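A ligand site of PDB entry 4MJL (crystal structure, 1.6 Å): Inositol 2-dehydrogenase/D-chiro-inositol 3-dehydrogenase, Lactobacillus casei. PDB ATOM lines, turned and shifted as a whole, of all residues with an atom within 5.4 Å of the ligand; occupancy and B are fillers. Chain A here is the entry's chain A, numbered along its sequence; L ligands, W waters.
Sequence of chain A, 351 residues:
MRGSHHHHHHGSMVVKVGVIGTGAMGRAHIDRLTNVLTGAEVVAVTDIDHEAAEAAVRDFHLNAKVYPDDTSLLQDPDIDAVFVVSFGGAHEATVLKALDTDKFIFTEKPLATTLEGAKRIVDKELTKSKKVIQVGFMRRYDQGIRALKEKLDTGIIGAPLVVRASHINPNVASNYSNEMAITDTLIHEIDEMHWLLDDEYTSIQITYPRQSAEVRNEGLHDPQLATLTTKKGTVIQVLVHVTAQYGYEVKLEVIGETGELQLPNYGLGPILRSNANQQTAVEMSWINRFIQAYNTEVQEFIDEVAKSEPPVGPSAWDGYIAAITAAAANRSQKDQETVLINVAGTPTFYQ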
ATOM      1  N   ILE A  20      -3.432  -4.541  14.973  1.00  0.00           N
ATOM      2  CA  ILE A  20      -3.180  -5.771  14.211  1.00  0.00           C
ATOM      3  C   ILE A  20      -3.647  -7.021  15.006  1.00  0.00           C
ATOM      4  O   ILE A  20      -2.955  -7.459  15.924  1.00  0.00           O
ATOM      5  CB  ILE A  20      -1.670  -5.845  13.932  1.00  0.00           C
ATOM      6  CG1 ILE A  20      -1.157  -4.586  13.190  1.00  0.00           C
ATOM      7  CG2 ILE A  20      -1.269  -7.163  13.225  1.00  0.00           C
ATOM      8  CD1 ILE A  20       0.311  -4.540  13.127  1.00  0.00           C
ATOM      9  N   GLY A  21      -4.789  -7.568  14.637  1.00  0.00           N
ATOM     10  CA  GLY A  21      -5.434  -8.674  15.346  1.00  0.00           C
ATOM     11  C   GLY A  21      -6.570  -8.099  16.121  1.00  0.00           C
ATOM     12  O   GLY A  21      -6.360  -7.490  17.176  1.00  0.00           O
ATOM     13  N   THR A  22      -7.774  -8.282  15.641  1.00  0.00           N
ATOM     14  CA  THR A  22      -8.979  -7.776  16.268  1.00  0.00           C
ATOM     15  C   THR A  22      -9.904  -8.908  16.804  1.00  0.00           C
ATOM     16  O   THR A  22     -11.084  -8.971  16.492  1.00  0.00           O
ATOM     17  CB  THR A  22      -9.753  -6.789  15.327  1.00  0.00           C
ATOM     18  OG1 THR A  22     -10.259  -7.533  14.231  1.00  0.00           O
ATOM     19  CG2 THR A  22      -8.822  -5.682  14.771  1.00  0.00           C
ATOM     20  N   GLY A  23      -9.330  -9.751  17.637  1.00  0.00           N
ATOM     21  CA  GLY A  23     -10.011 -10.865  18.292  1.00  0.00           C
ATOM     22  C   GLY A  23     -10.439 -10.434  19.685  1.00  0.00           C
ATOM     23  O   GLY A  23     -10.756  -9.277  19.883  1.00  0.00           O
ATOM     24  N   ALA A  24     -10.454 -11.354  20.645  1.00  0.00           N
ATOM     25  CA  ALA A  24     -10.985 -11.018  21.977  1.00  0.00           C
ATOM     26  C   ALA A  24     -10.107  -9.918  22.645  1.00  0.00           C
ATOM     27  O   ALA A  24     -10.658  -8.924  23.076  1.00  0.00           O
ATOM     28  CB  ALA A  24     -11.097 -12.272  22.920  1.00  0.00           C
ATOM     29  N   MET A  25      -8.805 -10.125  22.746  1.00  0.00           N
ATOM     30  CA  MET A  25      -7.952  -9.129  23.442  1.00  0.00           C
ATOM     31  C   MET A  25      -7.775  -7.880  22.558  1.00  0.00           C
ATOM     32  O   MET A  25      -7.727  -6.758  23.051  1.00  0.00           O
ATOM     33  CB  MET A  25      -6.595  -9.724  23.817  1.00  0.00           C
ATOM     34  CG  MET A  25      -5.692  -8.859  24.750  1.00  0.00           C
ATOM     35  SD  MET A  25      -6.679  -8.429  26.197  1.00  0.00           S
ATOM     36  CE  MET A  25      -5.347  -8.250  27.317  1.00  0.00           C
ATOM     37  N   GLY A  26      -7.724  -8.065  21.245  1.00  0.00           N
ATOM     38  CA  GLY A  26      -7.616  -6.925  20.358  1.00  0.00           C
ATOM     39  C   GLY A  26      -8.800  -6.014  20.521  1.00  0.00           C
ATOM     40  O   GLY A  26      -8.660  -4.792  20.608  1.00  0.00           O
ATOM     41  N   THR A  46      -6.304  -4.332  11.237  1.00  0.00           N
ATOM     42  CA  THR A  46      -6.149  -5.393  10.264  1.00  0.00           C
ATOM     43  C   THR A  46      -6.384  -6.701  11.003  1.00  0.00           C
ATOM     44  O   THR A  46      -6.030  -6.838  12.167  1.00  0.00           O
ATOM     45  CB  THR A  46      -4.783  -5.348   9.505  1.00  0.00           C
ATOM     46  OG1 THR A  46      -4.791  -6.353   8.456  1.00  0.00           O
ATOM     47  CG2 THR A  46      -3.567  -5.571  10.350  1.00  0.00           C
ATOM     48  N   ASP A  47      -6.903  -7.692  10.310  1.00  0.00           N
ATOM     49  CA  ASP A  47      -7.056  -9.033  10.873  1.00  0.00           C
ATOM     50  C   ASP A  47      -6.977 -10.024   9.664  1.00  0.00           C
ATOM     51  O   ASP A  47      -7.469  -9.663   8.568  1.00  0.00           O
ATOM     52  CB  ASP A  47      -8.399  -9.117  11.585  1.00  0.00           C
ATOM     53  CG  ASP A  47      -8.512 -10.324  12.481  1.00  0.00           C
ATOM     54  OD1 ASP A  47      -8.820 -11.432  11.998  1.00  0.00           O
ATOM     55  OD2 ASP A  47      -8.263 -10.218  13.715  1.00  0.00           O
ATOM     56  N   ILE A  48      -6.346 -11.192   9.826  1.00  0.00           N
ATOM     57  CA  ILE A  48      -6.386 -12.143   8.723  1.00  0.00           C
ATOM     58  C   ILE A  48      -7.789 -12.564   8.468  1.00  0.00           C
ATOM     59  O   ILE A  48      -8.071 -13.171   7.397  1.00  0.00           O
ATOM     60  CB  ILE A  48      -5.579 -13.364   8.983  1.00  0.00           C
ATOM     61  CG1 ILE A  48      -6.081 -14.130  10.230  1.00  0.00           C
ATOM     62  CG2 ILE A  48      -4.108 -13.043   8.954  1.00  0.00           C
ATOM     63  CD1 ILE A  48      -5.188 -15.323  10.536  1.00  0.00           C
ATOM     64  N   ASP A  49      -8.673 -12.326   9.427  1.00  0.00           N
ATOM     65  CA  ASP A  49     -10.082 -12.506   9.247  1.00  0.00           C
ATOM     66  C   ASP A  49     -10.774 -11.199   8.948  1.00  0.00           C
ATOM     67  O   ASP A  49     -11.299 -10.511   9.821  1.00  0.00           O
ATOM     68  CB  ASP A  49     -10.719 -13.241  10.417  1.00  0.00           C
ATOM     69  CG  ASP A  49     -12.219 -13.352  10.279  1.00  0.00           C
ATOM     70  OD1 ASP A  49     -12.765 -12.772   9.307  1.00  0.00           O
ATOM     71  OD2 ASP A  49     -12.880 -13.958  11.178  1.00  0.00           O
ATOM     72  N   ALA A  52     -13.507  -9.979  10.922  1.00  0.00           N
ATOM     73  CA  ALA A  52     -13.283  -9.601  12.330  1.00  0.00           C
ATOM     74  C   ALA A  52     -12.920  -8.106  12.298  1.00  0.00           C
ATOM     75  O   ALA A  52     -13.466  -7.304  13.065  1.00  0.00           O
ATOM     76  CB  ALA A  52     -12.180 -10.409  12.963  1.00  0.00           C
ATOM     77  N   VAL A  85      -1.850  -7.724  18.505  1.00  0.00           N
ATOM     78  CA  VAL A  85      -2.739  -8.555  19.296  1.00  0.00           C
ATOM     79  C   VAL A  85      -3.243  -9.790  18.535  1.00  0.00           C
ATOM     80  O   VAL A  85      -4.377 -10.235  18.723  1.00  0.00           O
ATOM     81  CB  VAL A  85      -3.927  -7.755  19.867  1.00  0.00           C
ATOM     82  CG1 VAL A  85      -4.366  -8.391  21.241  1.00  0.00           C
ATOM     83  CG2 VAL A  85      -3.519  -6.287  20.142  1.00  0.00           C
ATOM     84  N   SER A  86      -2.391 -10.290  17.667  1.00  0.00           N
ATOM     85  CA  SER A  86      -2.684 -11.477  16.857  1.00  0.00           C
ATOM     86  C   SER A  86      -2.338 -12.749  17.648  1.00  0.00           C
ATOM     87  O   SER A  86      -1.936 -12.674  18.831  1.00  0.00           O
ATOM     88  CB  SER A  86      -1.886 -11.371  15.549  1.00  0.00           C
ATOM     89  OG  SER A  86      -0.521 -11.156  15.765  1.00  0.00           O
ATOM     90  N   PHE A  87      -2.491 -13.928  17.046  1.00  0.00           N
ATOM     91  CA  PHE A  87      -1.993 -15.140  17.679  1.00  0.00           C
ATOM     92  C   PHE A  87      -0.579 -14.935  18.122  1.00  0.00           C
ATOM     93  O   PHE A  87       0.217 -14.273  17.447  1.00  0.00           O
ATOM     94  CB  PHE A  87      -1.980 -16.316  16.684  1.00  0.00           C
ATOM     95  CG  PHE A  87      -3.328 -16.708  16.117  1.00  0.00           C
ATOM     96  CD1 PHE A  87      -4.529 -16.460  16.779  1.00  0.00           C
ATOM     97  CD2 PHE A  87      -3.380 -17.364  14.844  1.00  0.00           C
ATOM     98  CE1 PHE A  87      -5.773 -16.803  16.223  1.00  0.00           C
ATOM     99  CE2 PHE A  87      -4.615 -17.731  14.290  1.00  0.00           C
ATOM    100  CZ  PHE A  87      -5.814 -17.480  14.974  1.00  0.00           C
ATOM    101  N   GLY A  88      -0.202 -15.532  19.257  1.00  0.00           N
ATOM    102  CA  GLY A  88       1.167 -15.429  19.731  1.00  0.00           C
ATOM    103  C   GLY A  88       2.238 -15.757  18.697  1.00  0.00           C
ATOM    104  O   GLY A  88       3.280 -15.075  18.621  1.00  0.00           O
ATOM    105  N   ALA A  90       2.229 -15.291  15.695  1.00  0.00           N
ATOM    106  CA  ALA A  90       2.244 -14.266  14.645  1.00  0.00           C
ATOM    107  C   ALA A  90       2.945 -12.959  15.079  1.00  0.00           C
ATOM    108  O   ALA A  90       3.071 -12.053  14.245  1.00  0.00           O
ATOM    109  CB  ALA A  90       0.868 -13.963  14.200  1.00  0.00           C
ATOM    110  N   HIS A  91       3.389 -12.856  16.354  1.00  0.00           N
ATOM    111  CA  HIS A  91       3.981 -11.586  16.834  1.00  0.00           C
ATOM    112  C   HIS A  91       5.338 -11.261  16.313  1.00  0.00           C
ATOM    113  O   HIS A  91       5.581 -10.126  15.916  1.00  0.00           O
ATOM    114  CB  HIS A  91       4.053 -11.522  18.394  1.00  0.00           C
ATOM    115  CG  HIS A  91       2.709 -11.567  19.056  1.00  0.00           C
ATOM    116  ND1 HIS A  91       2.562 -11.531  20.429  1.00  0.00           N
ATOM    117  CD2 HIS A  91       1.458 -11.657  18.538  1.00  0.00           C
ATOM    118  CE1 HIS A  91       1.273 -11.601  20.717  1.00  0.00           C
ATOM    119  NE2 HIS A  91       0.584 -11.693  19.610  1.00  0.00           N
ATOM    120  N   THR A  94       5.464  -9.843  12.769  1.00  0.00           N
ATOM    121  CA  THR A  94       4.785  -8.547  12.742  1.00  0.00           C
ATOM    122  C   THR A  94       5.625  -7.487  13.472  1.00  0.00           C
ATOM    123  O   THR A  94       5.709  -6.361  12.996  1.00  0.00           O
ATOM    124  CB  THR A  94       3.427  -8.584  13.354  1.00  0.00           C
ATOM    125  OG1 THR A  94       2.608  -9.407  12.548  1.00  0.00           O
ATOM    126  CG2 THR A  94       2.778  -7.183  13.352  1.00  0.00           C
ATOM    127  N   GLU A 108       1.188  -7.581  22.676  1.00  0.00           N
ATOM    128  CA  GLU A 108       0.767  -8.440  23.768  1.00  0.00           C
ATOM    129  C   GLU A 108       1.842  -9.480  23.948  1.00  0.00           C
ATOM    130  O   GLU A 108       2.657  -9.736  23.030  1.00  0.00           O
ATOM    131  CB  GLU A 108      -0.581  -9.095  23.436  1.00  0.00           C
ATOM    132  CG  GLU A 108      -1.779  -8.377  24.064  1.00  0.00           C
ATOM    133  CD  GLU A 108      -1.600  -8.182  25.580  1.00  0.00           C
ATOM    134  OE1 GLU A 108      -0.795  -8.925  26.211  1.00  0.00           O
ATOM    135  OE2 GLU A 108      -2.272  -7.290  26.098  1.00  0.00           O
ATOM    136  N   LYS A 109       1.866 -10.127  25.119  1.00  0.00           N
ATOM    137  CA  LYS A 109       2.712 -11.274  25.307  1.00  0.00           C
ATOM    138  C   LYS A 109       2.224 -12.381  24.390  1.00  0.00           C
ATOM    139  O   LYS A 109       1.044 -12.411  24.047  1.00  0.00           O
ATOM    140  CB  LYS A 109       2.732 -11.690  26.795  1.00  0.00           C
ATOM    141  CG  LYS A 109       1.400 -11.992  27.365  1.00  0.00           C
ATOM    142  CD  LYS A 109       1.087 -13.412  26.985  1.00  0.00           C
ATOM    143  CE  LYS A 109       0.144 -13.981  27.956  1.00  0.00           C
ATOM    144  NZ  LYS A 109      -0.676 -15.078  27.265  1.00  0.00           N
ATOM    145  N   PRO A 110       3.144 -13.273  23.951  1.00  0.00           N
ATOM    146  CA  PRO A 110       4.597 -13.246  24.190  1.00  0.00           C
ATOM    147  C   PRO A 110       5.304 -12.306  23.174  1.00  0.00           C
ATOM    148  O   PRO A 110       4.665 -11.966  22.154  1.00  0.00           O
ATOM    149  CB  PRO A 110       4.994 -14.697  23.893  1.00  0.00           C
ATOM    150  CG  PRO A 110       4.068 -15.077  22.858  1.00  0.00           C
ATOM    151  CD  PRO A 110       2.755 -14.482  23.204  1.00  0.00           C
ATOM    152  N   GLY A 136       3.029  -6.595  26.690  1.00  0.00           N
ATOM    153  CA  GLY A 136       1.863  -6.562  27.592  1.00  0.00           C
ATOM    154  C   GLY A 136       1.864  -7.387  28.882  1.00  0.00           C
ATOM    155  O   GLY A 136       0.867  -8.031  29.203  1.00  0.00           O
ATOM    156  N   MET A 138       1.020  -7.187  32.132  1.00  0.00           N
ATOM    157  CA  MET A 138       0.258  -6.226  32.936  1.00  0.00           C
ATOM    158  C   MET A 138       0.421  -6.378  34.446  1.00  0.00           C
ATOM    159  O   MET A 138       0.017  -5.501  35.166  1.00  0.00           O
ATOM    160  CB  MET A 138      -1.227  -6.259  32.569  1.00  0.00           C
ATOM    161  CG  MET A 138      -2.041  -7.414  33.229  1.00  0.00           C
ATOM    162  SD  MET A 138      -1.511  -9.036  32.650  1.00  0.00           S
ATOM    163  CE  MET A 138      -2.452 -10.134  33.763  1.00  0.00           C
ATOM    164  N   ASP A 184       0.713 -19.473  28.750  1.00  0.00           N
ATOM    165  CA  ASP A 184      -0.439 -18.597  28.973  1.00  0.00           C
ATOM    166  C   ASP A 184      -0.619 -18.196  30.467  1.00  0.00           C
ATOM    167  O   ASP A 184      -1.133 -17.124  30.786  1.00  0.00           O
ATOM    168  CB  ASP A 184      -1.734 -19.251  28.437  1.00  0.00           C
ATOM    169  CG  ASP A 184      -1.821 -19.212  26.861  1.00  0.00           C
ATOM    170  OD1 ASP A 184      -0.927 -18.596  26.196  1.00  0.00           O
ATOM    171  OD2 ASP A 184      -2.807 -19.727  26.292  1.00  0.00           O
ATOM    172  N   HIS A 188       3.062 -15.078  33.426  1.00  0.00           N
ATOM    173  CA  HIS A 188       2.883 -13.874  34.238  1.00  0.00           C
ATOM    174  C   HIS A 188       3.788 -13.837  35.440  1.00  0.00           C
ATOM    175  O   HIS A 188       4.385 -12.812  35.736  1.00  0.00           O
ATOM    176  CB  HIS A 188       1.403 -13.784  34.617  1.00  0.00           C
ATOM    177  CG  HIS A 188       0.533 -13.522  33.434  1.00  0.00           C
ATOM    178  ND1 HIS A 188       0.538 -12.304  32.783  1.00  0.00           N
ATOM    179  CD2 HIS A 188      -0.313 -14.322  32.754  1.00  0.00           C
ATOM    180  CE1 HIS A 188      -0.312 -12.357  31.764  1.00  0.00           C
ATOM    181  NE2 HIS A 188      -0.850 -13.565  31.728  1.00  0.00           N
ATOM    182  N   TRP A 286     -10.355 -13.965  35.351  1.00  0.00           N
ATOM    183  CA  TRP A 286      -9.090 -13.207  35.234  1.00  0.00           C
ATOM    184  C   TRP A 286      -9.263 -11.886  34.525  1.00  0.00           C
ATOM    185  O   TRP A 286      -8.524 -10.910  34.764  1.00  0.00           O
ATOM    186  CB  TRP A 286      -7.990 -14.000  34.576  1.00  0.00           C
ATOM    187  CG  TRP A 286      -8.341 -14.489  33.190  1.00  0.00           C
ATOM    188  CD1 TRP A 286      -8.868 -15.718  32.847  1.00  0.00           C
ATOM    189  CD2 TRP A 286      -8.117 -13.787  31.937  1.00  0.00           C
ATOM    190  NE1 TRP A 286      -9.026 -15.807  31.475  1.00  0.00           N
ATOM    191  CE2 TRP A 286      -8.567 -14.651  30.891  1.00  0.00           C
ATOM    192  CE3 TRP A 286      -7.657 -12.501  31.591  1.00  0.00           C
ATOM    193  CZ2 TRP A 286      -8.538 -14.275  29.535  1.00  0.00           C
ATOM    194  CZ3 TRP A 286      -7.600 -12.150  30.234  1.00  0.00           C
ATOM    195  CH2 TRP A 286      -8.038 -13.044  29.241  1.00  0.00           C
ATOM    196  N   TYR A 294      -4.660  -3.639  33.162  1.00  0.00           N
ATOM    197  CA  TYR A 294      -4.670  -3.395  31.707  1.00  0.00           C
ATOM    198  C   TYR A 294      -4.858  -1.920  31.383  1.00  0.00           C
ATOM    199  O   TYR A 294      -4.204  -1.412  30.493  1.00  0.00           O
ATOM    200  CB  TYR A 294      -5.762  -4.195  30.979  1.00  0.00           C
ATOM    201  CG  TYR A 294      -5.577  -5.688  31.052  1.00  0.00           C
ATOM    202  CD1 TYR A 294      -4.428  -6.303  30.571  1.00  0.00           C
ATOM    203  CD2 TYR A 294      -6.615  -6.487  31.491  1.00  0.00           C
ATOM    204  CE1 TYR A 294      -4.279  -7.692  30.598  1.00  0.00           C
ATOM    205  CE2 TYR A 294      -6.493  -7.848  31.540  1.00  0.00           C
ATOM    206  CZ  TYR A 294      -5.320  -8.456  31.092  1.00  0.00           C
ATOM    207  OH  TYR A 294      -5.248  -9.858  31.183  1.00  0.00           O
HETATM  208  P1  LIG L   1      -7.990 -14.404  19.480  1.00  0.00           P
HETATM  209  O1  LIG L   1      -7.724 -15.629  18.761  1.00  0.00           O
HETATM  210  O2  LIG L   1      -9.290 -14.084  19.876  1.00  0.00           O
HETATM  211  O3  LIG L   1      -7.691 -13.208  18.527  1.00  0.00           O
HETATM  212  C1  LIG L   1      -6.648 -13.162  17.649  1.00  0.00           C
HETATM  213  C2  LIG L   1      -7.012 -12.373  16.390  1.00  0.00           C
HETATM  214  O4  LIG L   1      -5.853 -12.265  15.634  1.00  0.00           O
HETATM  215  C3  LIG L   1      -7.967 -13.130  15.466  1.00  0.00           C
HETATM  216  O5  LIG L   1      -9.028 -12.326  15.074  1.00  0.00           O
HETATM  217  C4  LIG L   1      -7.077 -13.621  14.343  1.00  0.00           C
HETATM  218  O6  LIG L   1      -7.714 -13.801  13.106  1.00  0.00           O
HETATM  219  C5  LIG L   1      -6.123 -12.488  14.253  1.00  0.00           C
HETATM  220  N1  LIG L   1      -4.867 -12.819  13.600  1.00  0.00           N
HETATM  221  C6  LIG L   1      -4.227 -13.927  13.708  1.00  0.00           C
HETATM  222  N2  LIG L   1      -3.074 -13.899  13.062  1.00  0.00           N
HETATM  223  C7  LIG L   1      -2.992 -12.714  12.512  1.00  0.00           C
HETATM  224  C8  LIG L   1      -2.060 -12.034  11.654  1.00  0.00           C
HETATM  225  N3  LIG L   1      -0.937 -12.572  11.266  1.00  0.00           N
HETATM  226  N4  LIG L   1      -2.325 -10.791  11.348  1.00  0.00           N
HETATM  227  C9  LIG L   1      -3.418 -10.195  11.681  1.00  0.00           C
HETATM  228  N5  LIG L   1      -4.321 -10.767  12.437  1.00  0.00           N
HETATM  229  C10 LIG L   1      -4.166 -12.010  12.867  1.00  0.00           C
HETATM  230  O7  LIG L   1      -6.880 -14.335  20.585  1.00  0.00           O
HETATM  231  P2  LIG L   1      -6.704 -13.309  21.801  1.00  0.00           P
HETATM  232  O8  LIG L   1      -7.188 -13.936  23.011  1.00  0.00           O
HETATM  233  O9  LIG L   1      -7.358 -12.159  21.390  1.00  0.00           O
HETATM  234  O10 LIG L   1      -5.189 -13.260  21.927  1.00  0.00           O
HETATM  235  C11 LIG L   1      -4.431 -12.344  21.176  1.00  0.00           C
HETATM  236  C12 LIG L   1      -3.071 -12.118  21.789  1.00  0.00           C
HETATM  237  O11 LIG L   1      -3.266 -11.496  23.023  1.00  0.00           O
HETATM  238  C13 LIG L   1      -2.396 -13.409  22.106  1.00  0.00           C
HETATM  239  O12 LIG L   1      -1.047 -13.187  21.911  1.00  0.00           O
HETATM  240  C14 LIG L   1      -2.663 -13.609  23.583  1.00  0.00           C
HETATM  241  O13 LIG L   1      -1.596 -14.320  24.072  1.00  0.00           O
HETATM  242  C15 LIG L   1      -2.642 -12.184  24.068  1.00  0.00           C
HETATM  243  N6  LIG L   1      -3.353 -12.020  25.340  1.00  0.00           N
HETATM  244  C16 LIG L   1      -2.737 -11.506  26.389  1.00  0.00           C
HETATM  245  C17 LIG L   1      -3.386 -11.378  27.592  1.00  0.00           C
HETATM  246  C18 LIG L   1      -2.722 -10.793  28.791  1.00  0.00           C
HETATM  247  O14 LIG L   1      -3.160 -11.028  29.840  1.00  0.00           O
HETATM  248  N7  LIG L   1      -1.675 -10.053  28.607  1.00  0.00           N
HETATM  249  C19 LIG L   1      -4.716 -11.739  27.662  1.00  0.00           C
HETATM  250  C20 LIG L   1      -5.337 -12.253  26.549  1.00  0.00           C
HETATM  251  C21 LIG L   1      -4.593 -12.389  25.402  1.00  0.00           C
HETATM  252  O   HOH W   1      -1.501  -6.784  28.677  1.00  0.00           O
HETATM  253  O   HOH W   2       0.328 -10.206  13.520  1.00  0.00           O
HETATM  254  O   HOH W   3      -3.770  -8.949   8.808  1.00  0.00           O
HETATM  255  O   HOH W   4      -1.210  -9.423   9.013  1.00  0.00           O
HETATM  256  O   HOH W   5      -8.409 -13.399  25.468  1.00  0.00           O
HETATM  257  O   HOH W   6      -7.099 -10.250  19.385  1.00  0.00           O
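An oxygen (O5) of the ligand is in hydrogen-bond range of the side-chain carboxylate of Asp 47 (2.6 Å). An oxygen (O14) of the ligand is in hydrogen-bond range of the side-chain hydroxyl (OH) of Tyr 294 (2.7 Å). The side-chain carboxylate (OE1) of Glu 108 lies within hydrogen-bond range of a nitrogen (N7) of the ligand (2.8 Å). The backbone NH (N) of Met 25 is in hydrogen-bond range of an oxygen (O9) of the ligand. NE2 of His 91 lies close to O12 of the ligand (3.2 Å). The backbone NH of Ala 24 is in hydrogen-bond range of an oxygen (O2) of the ligand, at 3.1 Å. The backbone carbonyl oxygen (O) of Lys 109 is in hydrogen-bond range of an oxygen (O12) of the ligand (3.1 Å). The side-chain amino group of Lys 109 sits at hydrogen-bond distance from an oxygen (O13) of the ligand. The backbone carbonyl oxygen of Ser 86 sits close to an oxygen (O12) of the ligand (3.2 Å). The backbone carbonyl oxygen (O) of Gly 136 is in hydrogen-bond range of a nitrogen (N7) of the ligand. The backbone NH (N) of Ile 48 sits at hydrogen-bond distance from a nitrogen (N5) of the ligand (3.3 Å).
The side-chain carboxylate of Asp 47 sits at hydrogen-bond distance from the backbone NH of Thr 22, 2.8 Å away. The side-chain carboxylate (OD1) of Asp 47 lies within hydrogen-bond range of the backbone NH (N) of Asp 49. ND1 of His 91 lies within hydrogen-bond range of O of Glu 108 (3.2 Å). The backbone carbonyl oxygen (O) of Pro 110 sits at hydrogen-bond distance from a ring nitrogen (ND1) of His 91 (2.8 Å). The side-chain amino group (NZ) of Lys 109 lies within salt-bridge range of the side-chain carboxylate (OD1) of Asp 184 (3.7 Å). The backbone NH (N) of Ser 86 sits at hydrogen-bond distance from the backbone carbonyl oxygen (O) of Ile 20 (3.4 Å). N of Val 85 sits at hydrogen-bond distance from O of Ile 20 (2.8 Å). The backbone carbonyl oxygen (O) of Ala 90 lies within hydrogen-bond range of the side-chain hydroxyl (OG1) of Thr 94 (3.2 Å).
Residues that only touch the ligand: Gly 21 (3.6 Å), Thr 22 (3.9 Å), Gly 23 (3.3 Å), Val 85 (3.2 Å), Phe 87 (3.4 Å), Gly 88 (3.6 Å), Ala 90 (3.7 Å), Met 138 (3.8 Å), His 188 (3.7 Å) and Trp 286 (3.9 Å). Hydrophobic or aromatic side chains within 4 Å of the ligand: Ala 24, Met 25, Ile 48, Val 85, Phe 87, Ala 90, His 91, Met 138, His 188, Trp 286 and Tyr 294. The nearest printed residue that does not touch the ligand is Ile 20 (4.02 Å).
Water W6 lies within hydrogen-bond range of O9 of the ligand, O of Val 85, N of Gly 23 and N of Gly 26. Water W3 lies within hydrogen-bond range of OG1 of Thr 46 and N4 of the ligand. Water W1 lies within hydrogen-bond range of O of Gly 136, OE2 of Glu 108 and N7 of the ligand. Water W2 lies within hydrogen-bond range of OG of Ser 86 (2.6 Å), OG1 of Thr 94 (2.6 Å), O of Ala 90 (3.4 Å) and N4 of the ligand (3.5 Å).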
